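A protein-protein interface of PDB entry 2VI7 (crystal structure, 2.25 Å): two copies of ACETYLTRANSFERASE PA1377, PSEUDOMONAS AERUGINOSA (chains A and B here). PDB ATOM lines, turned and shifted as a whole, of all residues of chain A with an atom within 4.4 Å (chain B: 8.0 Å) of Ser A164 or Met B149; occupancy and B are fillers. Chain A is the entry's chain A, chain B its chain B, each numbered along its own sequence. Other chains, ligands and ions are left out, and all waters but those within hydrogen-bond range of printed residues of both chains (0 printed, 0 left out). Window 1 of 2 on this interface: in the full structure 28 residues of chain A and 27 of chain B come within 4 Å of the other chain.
NH1 of Arg A122 sits at hydrogen-bond distance from O of Arg B150 (2.7 Å).
The backbone carbonyl oxygen (O) of Glu A146 is in hydrogen-bond range of the backbone NH (N) of Glu B148.
The side-chain carboxylate (OE1) of Glu A146 lies within hydrogen-bond range of the backbone NH (N) of Arg B150 (3.2 Å).
The guanidinium group (NH2) of Arg A122 lies within salt-bridge range of the side-chain carboxylate (OE2) of Glu A146, at 2.8 Å.
The backbone NH (N) of Met A149 is in hydrogen-bond range of the backbone carbonyl oxygen (O) of Val A162, at 2.9 Å.
The backbone NH (N) of Glu B146 sits at hydrogen-bond distance from the backbone carbonyl oxygen (O) of Ser B164.
O of Gly B147 is in hydrogen-bond range of N of Ser B164, 2.9 Å away.
N of Met B149 is in hydrogen-bond range of O of Val B162 (2.9 Å).
The side-chain carboxylate of Asp B161 is in hydrogen-bond range of the backbone NH of Asp B151, at 3.0 Å.
Met B149 touches Arg A122.
Asp B151 touches Arg A122.
Gly B147 touches Glu A146 (CA to O, 3.0 Å).
OE2 of Glu A146 touches CA of Met B149, at 3.5 Å.
CA of Gly A147 touches O of Glu B146, at 3.1 Å.
Gly A147 touches Gly B147 (CA to CA, 3.6 Å).
CA of Met A149 touches OE1 of Glu B146 (3.6 Å).
OG of Ser A164 touches CE of Met B149 (3.3 Å).
Met B149 touches three residues of chain A.
Of the printed residues of chain B, Arg A122 touches Met B149 (3.4 Å), Arg B150 (2.7 Å) and Asp B151 (3.5 Å).
Printed residues of chain A within 4 Å of Arg B150: Arg A122 (2.7 Å) and Glu A146 (3.2 Å).
Of the printed residues of chain A, Glu B148 touches Glu A146.
Of the printed residues of chain A, Asp B151 touches Arg A122 (3.5 Å).
Printed residues of chain A within 4 Å of Glu B146: Gly A147 and Met A149.
Val B160 touches none of the printed residues of chain A.
Met A165 touches none of the printed residues of chain B.
The nearest residue of chain B that does not touch Ser A164 is Ser B164 (6.0 Å).
The nearest printed residue of chain A that does not touch Met B149 is Met A149 (5.9 Å).
Hydrophobic or aromatic side chains of chain B that line the printed part of chain A: Met B149.
Of the 11 printed residues of chain A, 5 touch a printed residue of chain B.
Printed residues of chain A that touch a printed residue of chain B: Arg A122, Glu A146, Gly A147, Met A149 and Ser A164.
Among the printed residues, 11 pairs touch across the chains.
Among the printed residues, no Asp or Glu carboxylate lies within 4 Å of a Lys or Arg side-chain nitrogen of the other chain.
Glu A146 touches Gly B147, and with the chains exchanged Gly A147 touches Glu B146.
Glu A146 touches Met B149, and with the chains exchanged Met A149 touches Glu B146.
Gly A147 touches its own counterpart, Gly B147.
Ser A164 touches Met B149, but with the chains exchanged Met A149 does not touch Ser B164 (4.4 Å).
Positions printed for both chains: 125, 145, 146, 147, 149, 162, 163, 164 and 165.
Of the 11 pairs that touch across the chains among the printed residues, 5 have their exchanged pair printed and touching as well.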
ATOM      1  N   ARG A 122     -29.774  12.382  -4.409  1.00  0.00           N
ATOM      2  CA  ARG A 122     -28.669  13.297  -4.182  1.00  0.00           C
ATOM      3  C   ARG A 122     -27.470  12.613  -3.546  1.00  0.00           C
ATOM      4  O   ARG A 122     -27.615  11.865  -2.584  1.00  0.00           O
ATOM      5  CB  ARG A 122     -29.175  14.417  -3.268  1.00  0.00           C
ATOM      6  CG  ARG A 122     -28.177  15.466  -2.860  1.00  0.00           C
ATOM      7  CD  ARG A 122     -28.801  16.384  -1.823  1.00  0.00           C
ATOM      8  NE  ARG A 122     -27.781  17.219  -1.196  1.00  0.00           N
ATOM      9  CZ  ARG A 122     -27.276  18.318  -1.745  1.00  0.00           C
ATOM     10  NH1 ARG A 122     -27.711  18.726  -2.926  1.00  0.00           N
ATOM     11  NH2 ARG A 122     -26.303  18.982  -1.141  1.00  0.00           N
ATOM     12  N   LEU A 125     -20.458  15.281  -1.481  1.00  0.00           N
ATOM     13  CA  LEU A 125     -19.039  15.090  -1.211  1.00  0.00           C
ATOM     14  C   LEU A 125     -18.368  16.432  -0.983  1.00  0.00           C
ATOM     15  O   LEU A 125     -18.951  17.478  -1.245  1.00  0.00           O
ATOM     16  CB  LEU A 125     -18.356  14.371  -2.385  1.00  0.00           C
ATOM     17  CG  LEU A 125     -18.136  15.103  -3.721  1.00  0.00           C
ATOM     18  CD1 LEU A 125     -17.081  16.184  -3.578  1.00  0.00           C
ATOM     19  CD2 LEU A 125     -17.685  14.096  -4.764  1.00  0.00           C
ATOM     20  N   GLU A 144     -21.511  18.815  -9.148  1.00  0.00           N
ATOM     21  CA  GLU A 144     -21.357  20.228  -9.391  1.00  0.00           C
ATOM     22  C   GLU A 144     -21.040  20.877  -8.065  1.00  0.00           C
ATOM     23  O   GLU A 144     -21.494  20.414  -7.024  1.00  0.00           O
ATOM     24  CB  GLU A 144     -22.640  20.821  -9.939  1.00  0.00           C
ATOM     25  CG  GLU A 144     -23.026  20.344 -11.313  1.00  0.00           C
ATOM     26  CD  GLU A 144     -24.332  20.979 -11.772  1.00  0.00           C
ATOM     27  OE1 GLU A 144     -24.370  22.221 -11.961  1.00  0.00           O
ATOM     28  OE2 GLU A 144     -25.321  20.234 -11.929  1.00  0.00           O
ATOM     29  N   THR A 145     -20.257  21.949  -8.106  1.00  0.00           N
ATOM     30  CA  THR A 145     -19.889  22.672  -6.902  1.00  0.00           C
ATOM     31  C   THR A 145     -21.098  23.434  -6.382  1.00  0.00           C
ATOM     32  O   THR A 145     -21.746  24.174  -7.125  1.00  0.00           O
ATOM     33  CB  THR A 145     -18.755  23.675  -7.178  1.00  0.00           C
ATOM     34  OG1 THR A 145     -17.576  22.964  -7.576  1.00  0.00           O
ATOM     35  CG2 THR A 145     -18.456  24.506  -5.931  1.00  0.00           C
ATOM     36  N   GLU A 146     -21.395  23.247  -5.101  1.00  0.00           N
ATOM     37  CA  GLU A 146     -22.521  23.909  -4.468  1.00  0.00           C
ATOM     38  C   GLU A 146     -22.060  24.974  -3.492  1.00  0.00           C
ATOM     39  O   GLU A 146     -22.829  25.851  -3.111  1.00  0.00           O
ATOM     40  CB  GLU A 146     -23.393  22.889  -3.743  1.00  0.00           C
ATOM     41  CG  GLU A 146     -24.318  22.119  -4.661  1.00  0.00           C
ATOM     42  CD  GLU A 146     -25.340  21.302  -3.901  1.00  0.00           C
ATOM     43  OE1 GLU A 146     -26.407  20.999  -4.481  1.00  0.00           O
ATOM     44  OE2 GLU A 146     -25.072  20.958  -2.730  1.00  0.00           O
ATOM     45  N   GLY A 147     -20.802  24.903  -3.086  1.00  0.00           N
ATOM     46  CA  GLY A 147     -20.298  25.888  -2.155  1.00  0.00           C
ATOM     47  C   GLY A 147     -18.831  25.700  -1.870  1.00  0.00           C
ATOM     48  O   GLY A 147     -18.257  24.673  -2.214  1.00  0.00           O
ATOM     49  N   MET A 149     -16.197  26.026   1.356  1.00  0.00           N
ATOM     50  CA  MET A 149     -16.103  26.131   2.804  1.00  0.00           C
ATOM     51  C   MET A 149     -14.690  26.435   3.302  1.00  0.00           C
ATOM     52  O   MET A 149     -13.782  25.618   3.181  1.00  0.00           O
ATOM     53  CB  MET A 149     -16.645  24.839   3.401  1.00  0.00           C
ATOM     54  CG  MET A 149     -17.851  24.352   2.615  1.00  0.00           C
ATOM     55  SD  MET A 149     -18.951  23.298   3.533  1.00  0.00           S
ATOM     56  CE  MET A 149     -18.390  21.704   3.015  1.00  0.00           C
ATOM     57  N   VAL A 162     -12.507  23.637   1.099  1.00  0.00           N
ATOM     58  CA  VAL A 162     -13.015  22.539   0.299  1.00  0.00           C
ATOM     59  C   VAL A 162     -14.195  23.035  -0.502  1.00  0.00           C
ATOM     60  O   VAL A 162     -14.797  24.055  -0.182  1.00  0.00           O
ATOM     61  CB  VAL A 162     -13.534  21.333   1.150  1.00  0.00           C
ATOM     62  CG1 VAL A 162     -12.453  20.831   2.084  1.00  0.00           C
ATOM     63  CG2 VAL A 162     -14.800  21.724   1.910  1.00  0.00           C
ATOM     64  N   TYR A 163     -14.496  22.309  -1.564  1.00  0.00           N
ATOM     65  CA  TYR A 163     -15.655  22.600  -2.382  1.00  0.00           C
ATOM     66  C   TYR A 163     -16.691  21.574  -1.932  1.00  0.00           C
ATOM     67  O   TYR A 163     -16.385  20.389  -1.772  1.00  0.00           O
ATOM     68  CB  TYR A 163     -15.354  22.400  -3.869  1.00  0.00           C
ATOM     69  CG  TYR A 163     -14.578  23.532  -4.489  1.00  0.00           C
ATOM     70  CD1 TYR A 163     -13.474  23.293  -5.297  1.00  0.00           C
ATOM     71  CD2 TYR A 163     -14.955  24.850  -4.270  1.00  0.00           C
ATOM     72  CE1 TYR A 163     -12.762  24.349  -5.871  1.00  0.00           C
ATOM     73  CE2 TYR A 163     -14.250  25.911  -4.839  1.00  0.00           C
ATOM     74  CZ  TYR A 163     -13.154  25.653  -5.635  1.00  0.00           C
ATOM     75  OH  TYR A 163     -12.451  26.712  -6.173  1.00  0.00           O
ATOM     76  N   SER A 164     -17.902  22.040  -1.682  1.00  0.00           N
ATOM     77  CA  SER A 164     -18.988  21.159  -1.292  1.00  0.00           C
ATOM     78  C   SER A 164     -19.687  20.843  -2.613  1.00  0.00           C
ATOM     79  O   SER A 164     -20.195  21.746  -3.263  1.00  0.00           O
ATOM     80  CB  SER A 164     -19.939  21.894  -0.354  1.00  0.00           C
ATOM     81  OG  SER A 164     -20.932  21.011   0.122  1.00  0.00           O
ATOM     82  N   MET A 165     -19.691  19.576  -3.020  1.00  0.00           N
ATOM     83  CA  MET A 165     -20.319  19.195  -4.276  1.00  0.00           C
ATOM     84  C   MET A 165     -21.479  18.224  -4.121  1.00  0.00           C
ATOM     85  O   MET A 165     -21.591  17.512  -3.133  1.00  0.00           O
ATOM     86  CB  MET A 165     -19.286  18.590  -5.215  1.00  0.00           C
ATOM     87  CG  MET A 165     -18.103  19.504  -5.508  1.00  0.00           C
ATOM     88  SD  MET A 165     -16.929  18.699  -6.587  1.00  0.00           S
ATOM     89  CE  MET A 165     -17.555  19.207  -8.184  1.00  0.00           C
ATOM     90  N   LEU B 125     -23.689  25.809  10.058  1.00  0.00           N
ATOM     91  CA  LEU B 125     -25.131  25.598  10.204  1.00  0.00           C
ATOM     92  C   LEU B 125     -25.770  25.510   8.827  1.00  0.00           C
ATOM     93  O   LEU B 125     -25.145  25.850   7.831  1.00  0.00           O
ATOM     94  CB  LEU B 125     -25.786  26.731  11.010  1.00  0.00           C
ATOM     95  CG  LEU B 125     -25.971  28.108  10.374  1.00  0.00           C
ATOM     96  CD1 LEU B 125     -27.095  28.089   9.360  1.00  0.00           C
ATOM     97  CD2 LEU B 125     -26.299  29.094  11.455  1.00  0.00           C
ATOM     98  N   THR B 126     -26.998  25.015   8.764  1.00  0.00           N
ATOM     99  CA  THR B 126     -27.731  24.935   7.497  1.00  0.00           C
ATOM    100  C   THR B 126     -29.089  25.557   7.765  1.00  0.00           C
ATOM    101  O   THR B 126     -29.624  25.470   8.874  1.00  0.00           O
ATOM    102  CB  THR B 126     -27.934  23.488   6.979  1.00  0.00           C
ATOM    103  OG1 THR B 126     -28.440  22.668   8.033  1.00  0.00           O
ATOM    104  CG2 THR B 126     -26.628  22.909   6.447  1.00  0.00           C
ATOM    105  N   VAL B 127     -29.651  26.198   6.759  1.00  0.00           N
ATOM    106  CA  VAL B 127     -30.930  26.855   6.949  1.00  0.00           C
ATOM    107  C   VAL B 127     -31.682  26.805   5.638  1.00  0.00           C
ATOM    108  O   VAL B 127     -31.081  26.942   4.573  1.00  0.00           O
ATOM    109  CB  VAL B 127     -30.710  28.343   7.410  1.00  0.00           C
ATOM    110  CG1 VAL B 127     -29.848  29.088   6.391  1.00  0.00           C
ATOM    111  CG2 VAL B 127     -32.048  29.054   7.614  1.00  0.00           C
ATOM    112  N   TYR B 128     -32.990  26.579   5.708  1.00  0.00           N
ATOM    113  CA  TYR B 128     -33.800  26.537   4.496  1.00  0.00           C
ATOM    114  C   TYR B 128     -33.710  27.903   3.820  1.00  0.00           C
ATOM    115  O   TYR B 128     -33.849  28.936   4.472  1.00  0.00           O
ATOM    116  CB  TYR B 128     -35.245  26.181   4.855  1.00  0.00           C
ATOM    117  CG  TYR B 128     -35.408  24.725   5.254  1.00  0.00           C
ATOM    118  CD1 TYR B 128     -35.940  24.367   6.490  1.00  0.00           C
ATOM    119  CD2 TYR B 128     -34.986  23.703   4.404  1.00  0.00           C
ATOM    120  CE1 TYR B 128     -36.037  23.023   6.872  1.00  0.00           C
ATOM    121  CE2 TYR B 128     -35.079  22.362   4.777  1.00  0.00           C
ATOM    122  CZ  TYR B 128     -35.603  22.031   6.011  1.00  0.00           C
ATOM    123  OH  TYR B 128     -35.679  20.702   6.381  1.00  0.00           O
ATOM    124  N   THR B 129     -33.461  27.900   2.516  1.00  0.00           N
ATOM    125  CA  THR B 129     -33.311  29.145   1.762  1.00  0.00           C
ATOM    126  C   THR B 129     -34.445  30.167   1.878  1.00  0.00           C
ATOM    127  O   THR B 129     -34.216  31.358   1.688  1.00  0.00           O
ATOM    128  CB  THR B 129     -33.078  28.863   0.255  1.00  0.00           C
ATOM    129  OG1 THR B 129     -34.245  28.258  -0.310  1.00  0.00           O
ATOM    130  CG2 THR B 129     -31.890  27.939   0.060  1.00  0.00           C
ATOM    131  N   THR B 145     -23.229  32.969   3.978  1.00  0.00           N
ATOM    132  CA  THR B 145     -23.600  31.849   3.133  1.00  0.00           C
ATOM    133  C   THR B 145     -22.378  31.391   2.362  1.00  0.00           C
ATOM    134  O   THR B 145     -21.673  32.193   1.754  1.00  0.00           O
ATOM    135  CB  THR B 145     -24.719  32.242   2.161  1.00  0.00           C
ATOM    136  OG1 THR B 145     -25.863  32.662   2.914  1.00  0.00           O
ATOM    137  CG2 THR B 145     -25.107  31.065   1.287  1.00  0.00           C
ATOM    138  N   GLU B 146     -22.126  30.091   2.407  1.00  0.00           N
ATOM    139  CA  GLU B 146     -20.981  29.498   1.727  1.00  0.00           C
ATOM    140  C   GLU B 146     -21.416  28.655   0.541  1.00  0.00           C
ATOM    141  O   GLU B 146     -20.649  28.448  -0.403  1.00  0.00           O
ATOM    142  CB  GLU B 146     -20.195  28.609   2.690  1.00  0.00           C
ATOM    143  CG  GLU B 146     -19.356  29.346   3.707  1.00  0.00           C
ATOM    144  CD  GLU B 146     -18.500  28.402   4.523  1.00  0.00           C
ATOM    145  OE1 GLU B 146     -17.378  28.795   4.897  1.00  0.00           O
ATOM    146  OE2 GLU B 146     -18.954  27.272   4.794  1.00  0.00           O
ATOM    147  N   GLY B 147     -22.644  28.151   0.604  1.00  0.00           N
ATOM    148  CA  GLY B 147     -23.147  27.330  -0.474  1.00  0.00           C
ATOM    149  C   GLY B 147     -24.648  27.187  -0.432  1.00  0.00           C
ATOM    150  O   GLY B 147     -25.290  27.508   0.567  1.00  0.00           O
ATOM    151  N   GLU B 148     -25.207  26.715  -1.538  1.00  0.00           N
ATOM    152  CA  GLU B 148     -26.638  26.497  -1.645  1.00  0.00           C
ATOM    153  C   GLU B 148     -26.796  25.041  -2.059  1.00  0.00           C
ATOM    154  O   GLU B 148     -26.266  24.612  -3.076  1.00  0.00           O
ATOM    155  CB  GLU B 148     -27.243  27.434  -2.688  1.00  0.00           C
ATOM    156  CG  GLU B 148     -28.756  27.361  -2.768  1.00  0.00           C
ATOM    157  CD  GLU B 148     -29.369  28.540  -3.509  1.00  0.00           C
ATOM    158  OE1 GLU B 148     -30.612  28.626  -3.562  1.00  0.00           O
ATOM    159  OE2 GLU B 148     -28.612  29.380  -4.038  1.00  0.00           O
ATOM    160  N   MET B 149     -27.529  24.277  -1.266  1.00  0.00           N
ATOM    161  CA  MET B 149     -27.694  22.864  -1.541  1.00  0.00           C
ATOM    162  C   MET B 149     -29.101  22.516  -1.991  1.00  0.00           C
ATOM    163  O   MET B 149     -30.066  22.665  -1.242  1.00  0.00           O
ATOM    164  CB  MET B 149     -27.296  22.098  -0.290  1.00  0.00           C
ATOM    165  CG  MET B 149     -26.072  22.714   0.330  1.00  0.00           C
ATOM    166  SD  MET B 149     -25.604  21.958   1.853  1.00  0.00           S
ATOM    167  CE  MET B 149     -24.034  21.238   1.358  1.00  0.00           C
ATOM    168  N   ARG B 150     -29.189  22.049  -3.232  1.00  0.00           N
ATOM    169  CA  ARG B 150     -30.441  21.682  -3.879  1.00  0.00           C
ATOM    170  C   ARG B 150     -31.040  20.362  -3.403  1.00  0.00           C
ATOM    171  O   ARG B 150     -30.329  19.378  -3.223  1.00  0.00           O
ATOM    172  CB  ARG B 150     -30.220  21.620  -5.391  1.00  0.00           C
ATOM    173  CG  ARG B 150     -29.612  22.881  -5.978  1.00  0.00           C
ATOM    174  CD  ARG B 150     -30.462  24.094  -5.632  1.00  0.00           C
ATOM    175  NE  ARG B 150     -29.994  25.321  -6.273  1.00  0.00           N
ATOM    176  CZ  ARG B 150     -30.636  26.488  -6.217  1.00  0.00           C
ATOM    177  N   ASP B 151     -32.360  20.354  -3.223  1.00  0.00           N
ATOM    178  CA  ASP B 151     -33.090  19.169  -2.777  1.00  0.00           C
ATOM    179  C   ASP B 151     -32.361  18.515  -1.613  1.00  0.00           C
ATOM    180  O   ASP B 151     -32.154  17.302  -1.589  1.00  0.00           O
ATOM    181  CB  ASP B 151     -33.229  18.166  -3.923  1.00  0.00           C
ATOM    182  CG  ASP B 151     -33.982  18.735  -5.106  1.00  0.00           C
ATOM    183  OD1 ASP B 151     -34.597  19.817  -4.983  1.00  0.00           O
ATOM    184  OD2 ASP B 151     -33.971  18.086  -6.168  1.00  0.00           O
ATOM    185  N   TYR B 152     -31.979  19.339  -0.646  1.00  0.00           N
ATOM    186  CA  TYR B 152     -31.254  18.886   0.533  1.00  0.00           C
ATOM    187  C   TYR B 152     -32.118  18.039   1.452  1.00  0.00           C
ATOM    188  O   TYR B 152     -31.708  16.971   1.892  1.00  0.00           O
ATOM    189  CB  TYR B 152     -30.742  20.091   1.316  1.00  0.00           C
ATOM    190  CG  TYR B 152     -29.829  19.740   2.474  1.00  0.00           C
ATOM    191  CD1 TYR B 152     -28.516  19.337   2.250  1.00  0.00           C
ATOM    192  CD2 TYR B 152     -30.268  19.846   3.797  1.00  0.00           C
ATOM    193  CE1 TYR B 152     -27.654  19.058   3.315  1.00  0.00           C
ATOM    194  CE2 TYR B 152     -29.416  19.565   4.867  1.00  0.00           C
ATOM    195  CZ  TYR B 152     -28.113  19.177   4.618  1.00  0.00           C
ATOM    196  OH  TYR B 152     -27.260  18.936   5.672  1.00  0.00           O
ATOM    197  N   ALA B 153     -33.312  18.530   1.748  1.00  0.00           N
ATOM    198  CA  ALA B 153     -34.204  17.816   2.641  1.00  0.00           C
ATOM    199  C   ALA B 153     -35.667  17.879   2.224  1.00  0.00           C
ATOM    200  O   ALA B 153     -36.062  18.666   1.360  1.00  0.00           O
ATOM    201  CB  ALA B 153     -34.045  18.356   4.063  1.00  0.00           C
ATOM    202  N   PHE B 159     -38.836  18.208  -1.917  1.00  0.00           N
ATOM    203  CA  PHE B 159     -37.439  18.469  -1.620  1.00  0.00           C
ATOM    204  C   PHE B 159     -37.174  19.961  -1.682  1.00  0.00           C
ATOM    205  O   PHE B 159     -37.512  20.618  -2.669  1.00  0.00           O
ATOM    206  CB  PHE B 159     -36.558  17.742  -2.622  1.00  0.00           C
ATOM    207  CG  PHE B 159     -36.775  16.264  -2.643  1.00  0.00           C
ATOM    208  CD1 PHE B 159     -37.348  15.655  -3.746  1.00  0.00           C
ATOM    209  CD2 PHE B 159     -36.405  15.475  -1.558  1.00  0.00           C
ATOM    210  CE1 PHE B 159     -37.554  14.280  -3.771  1.00  0.00           C
ATOM    211  CE2 PHE B 159     -36.607  14.102  -1.573  1.00  0.00           C
ATOM    212  CZ  PHE B 159     -37.180  13.501  -2.682  1.00  0.00           C
ATOM    213  N   VAL B 160     -36.572  20.498  -0.627  1.00  0.00           N
ATOM    214  CA  VAL B 160     -36.278  21.923  -0.568  1.00  0.00           C
ATOM    215  C   VAL B 160     -34.777  22.198  -0.401  1.00  0.00           C
ATOM    216  O   VAL B 160     -34.001  21.309  -0.044  1.00  0.00           O
ATOM    217  CB  VAL B 160     -37.076  22.590   0.577  1.00  0.00           C
ATOM    218  CG1 VAL B 160     -38.564  22.386   0.351  1.00  0.00           C
ATOM    219  CG2 VAL B 160     -36.685  21.986   1.907  1.00  0.00           C
ATOM    220  N   ASP B 161     -34.370  23.432  -0.675  1.00  0.00           N
ATOM    221  CA  ASP B 161     -32.965  23.803  -0.567  1.00  0.00           C
ATOM    222  C   ASP B 161     -32.613  24.450   0.768  1.00  0.00           C
ATOM    223  O   ASP B 161     -33.461  25.016   1.458  1.00  0.00           O
ATOM    224  CB  ASP B 161     -32.564  24.793  -1.676  1.00  0.00           C
ATOM    225  CG  ASP B 161     -33.096  24.409  -3.048  1.00  0.00           C
ATOM    226  OD1 ASP B 161     -33.097  23.206  -3.391  1.00  0.00           O
ATOM    227  OD2 ASP B 161     -33.498  25.329  -3.794  1.00  0.00           O
ATOM    228  N   VAL B 162     -31.341  24.362   1.121  1.00  0.00           N
ATOM    229  CA  VAL B 162     -30.867  24.990   2.337  1.00  0.00           C
ATOM    230  C   VAL B 162     -29.593  25.755   2.012  1.00  0.00           C
ATOM    231  O   VAL B 162     -28.882  25.438   1.063  1.00  0.00           O
ATOM    232  CB  VAL B 162     -30.528  23.964   3.470  1.00  0.00           C
ATOM    233  CG1 VAL B 162     -31.720  23.096   3.779  1.00  0.00           C
ATOM    234  CG2 VAL B 162     -29.345  23.122   3.069  1.00  0.00           C
ATOM    235  N   TYR B 163     -29.330  26.793   2.789  1.00  0.00           N
ATOM    236  CA  TYR B 163     -28.102  27.539   2.628  1.00  0.00           C
ATOM    237  C   TYR B 163     -27.177  26.946   3.686  1.00  0.00           C
ATOM    238  O   TYR B 163     -27.601  26.628   4.802  1.00  0.00           O
ATOM    239  CB  TYR B 163     -28.307  29.027   2.920  1.00  0.00           C
ATOM    240  CG  TYR B 163     -28.942  29.830   1.804  1.00  0.00           C
ATOM    241  CD1 TYR B 163     -30.034  30.664   2.063  1.00  0.00           C
ATOM    242  CD2 TYR B 163     -28.426  29.802   0.511  1.00  0.00           C
ATOM    243  CE1 TYR B 163     -30.590  31.447   1.067  1.00  0.00           C
ATOM    244  CE2 TYR B 163     -28.974  30.583  -0.488  1.00  0.00           C
ATOM    245  CZ  TYR B 163     -30.054  31.403  -0.203  1.00  0.00           C
ATOM    246  OH  TYR B 163     -30.592  32.188  -1.192  1.00  0.00           O
ATOM    247  N   SER B 164     -25.919  26.772   3.314  1.00  0.00           N
ATOM    248  CA  SER B 164     -24.906  26.249   4.211  1.00  0.00           C
ATOM    249  C   SER B 164     -24.185  27.496   4.673  1.00  0.00           C
ATOM    250  O   SER B 164     -23.672  28.238   3.848  1.00  0.00           O
ATOM    251  CB  SER B 164     -23.947  25.355   3.440  1.00  0.00           C
ATOM    252  OG  SER B 164     -23.052  24.728   4.328  1.00  0.00           O
ATOM    253  N   MET B 165     -24.149  27.742   5.974  1.00  0.00           N
ATOM    254  CA  MET B 165     -23.501  28.946   6.473  1.00  0.00           C
ATOM    255  C   MET B 165     -22.389  28.649   7.450  1.00  0.00           C
ATOM    256  O   MET B 165     -22.333  27.574   8.032  1.00  0.00           O
ATOM    257  CB  MET B 165     -24.523  29.851   7.152  1.00  0.00           C
ATOM    258  CG  MET B 165     -25.684  30.248   6.270  1.00  0.00           C
ATOM    259  SD  MET B 165     -26.810  31.328   7.155  1.00  0.00           S
ATOM    260  CE  MET B 165     -26.218  32.926   6.673  1.00  0.00           C
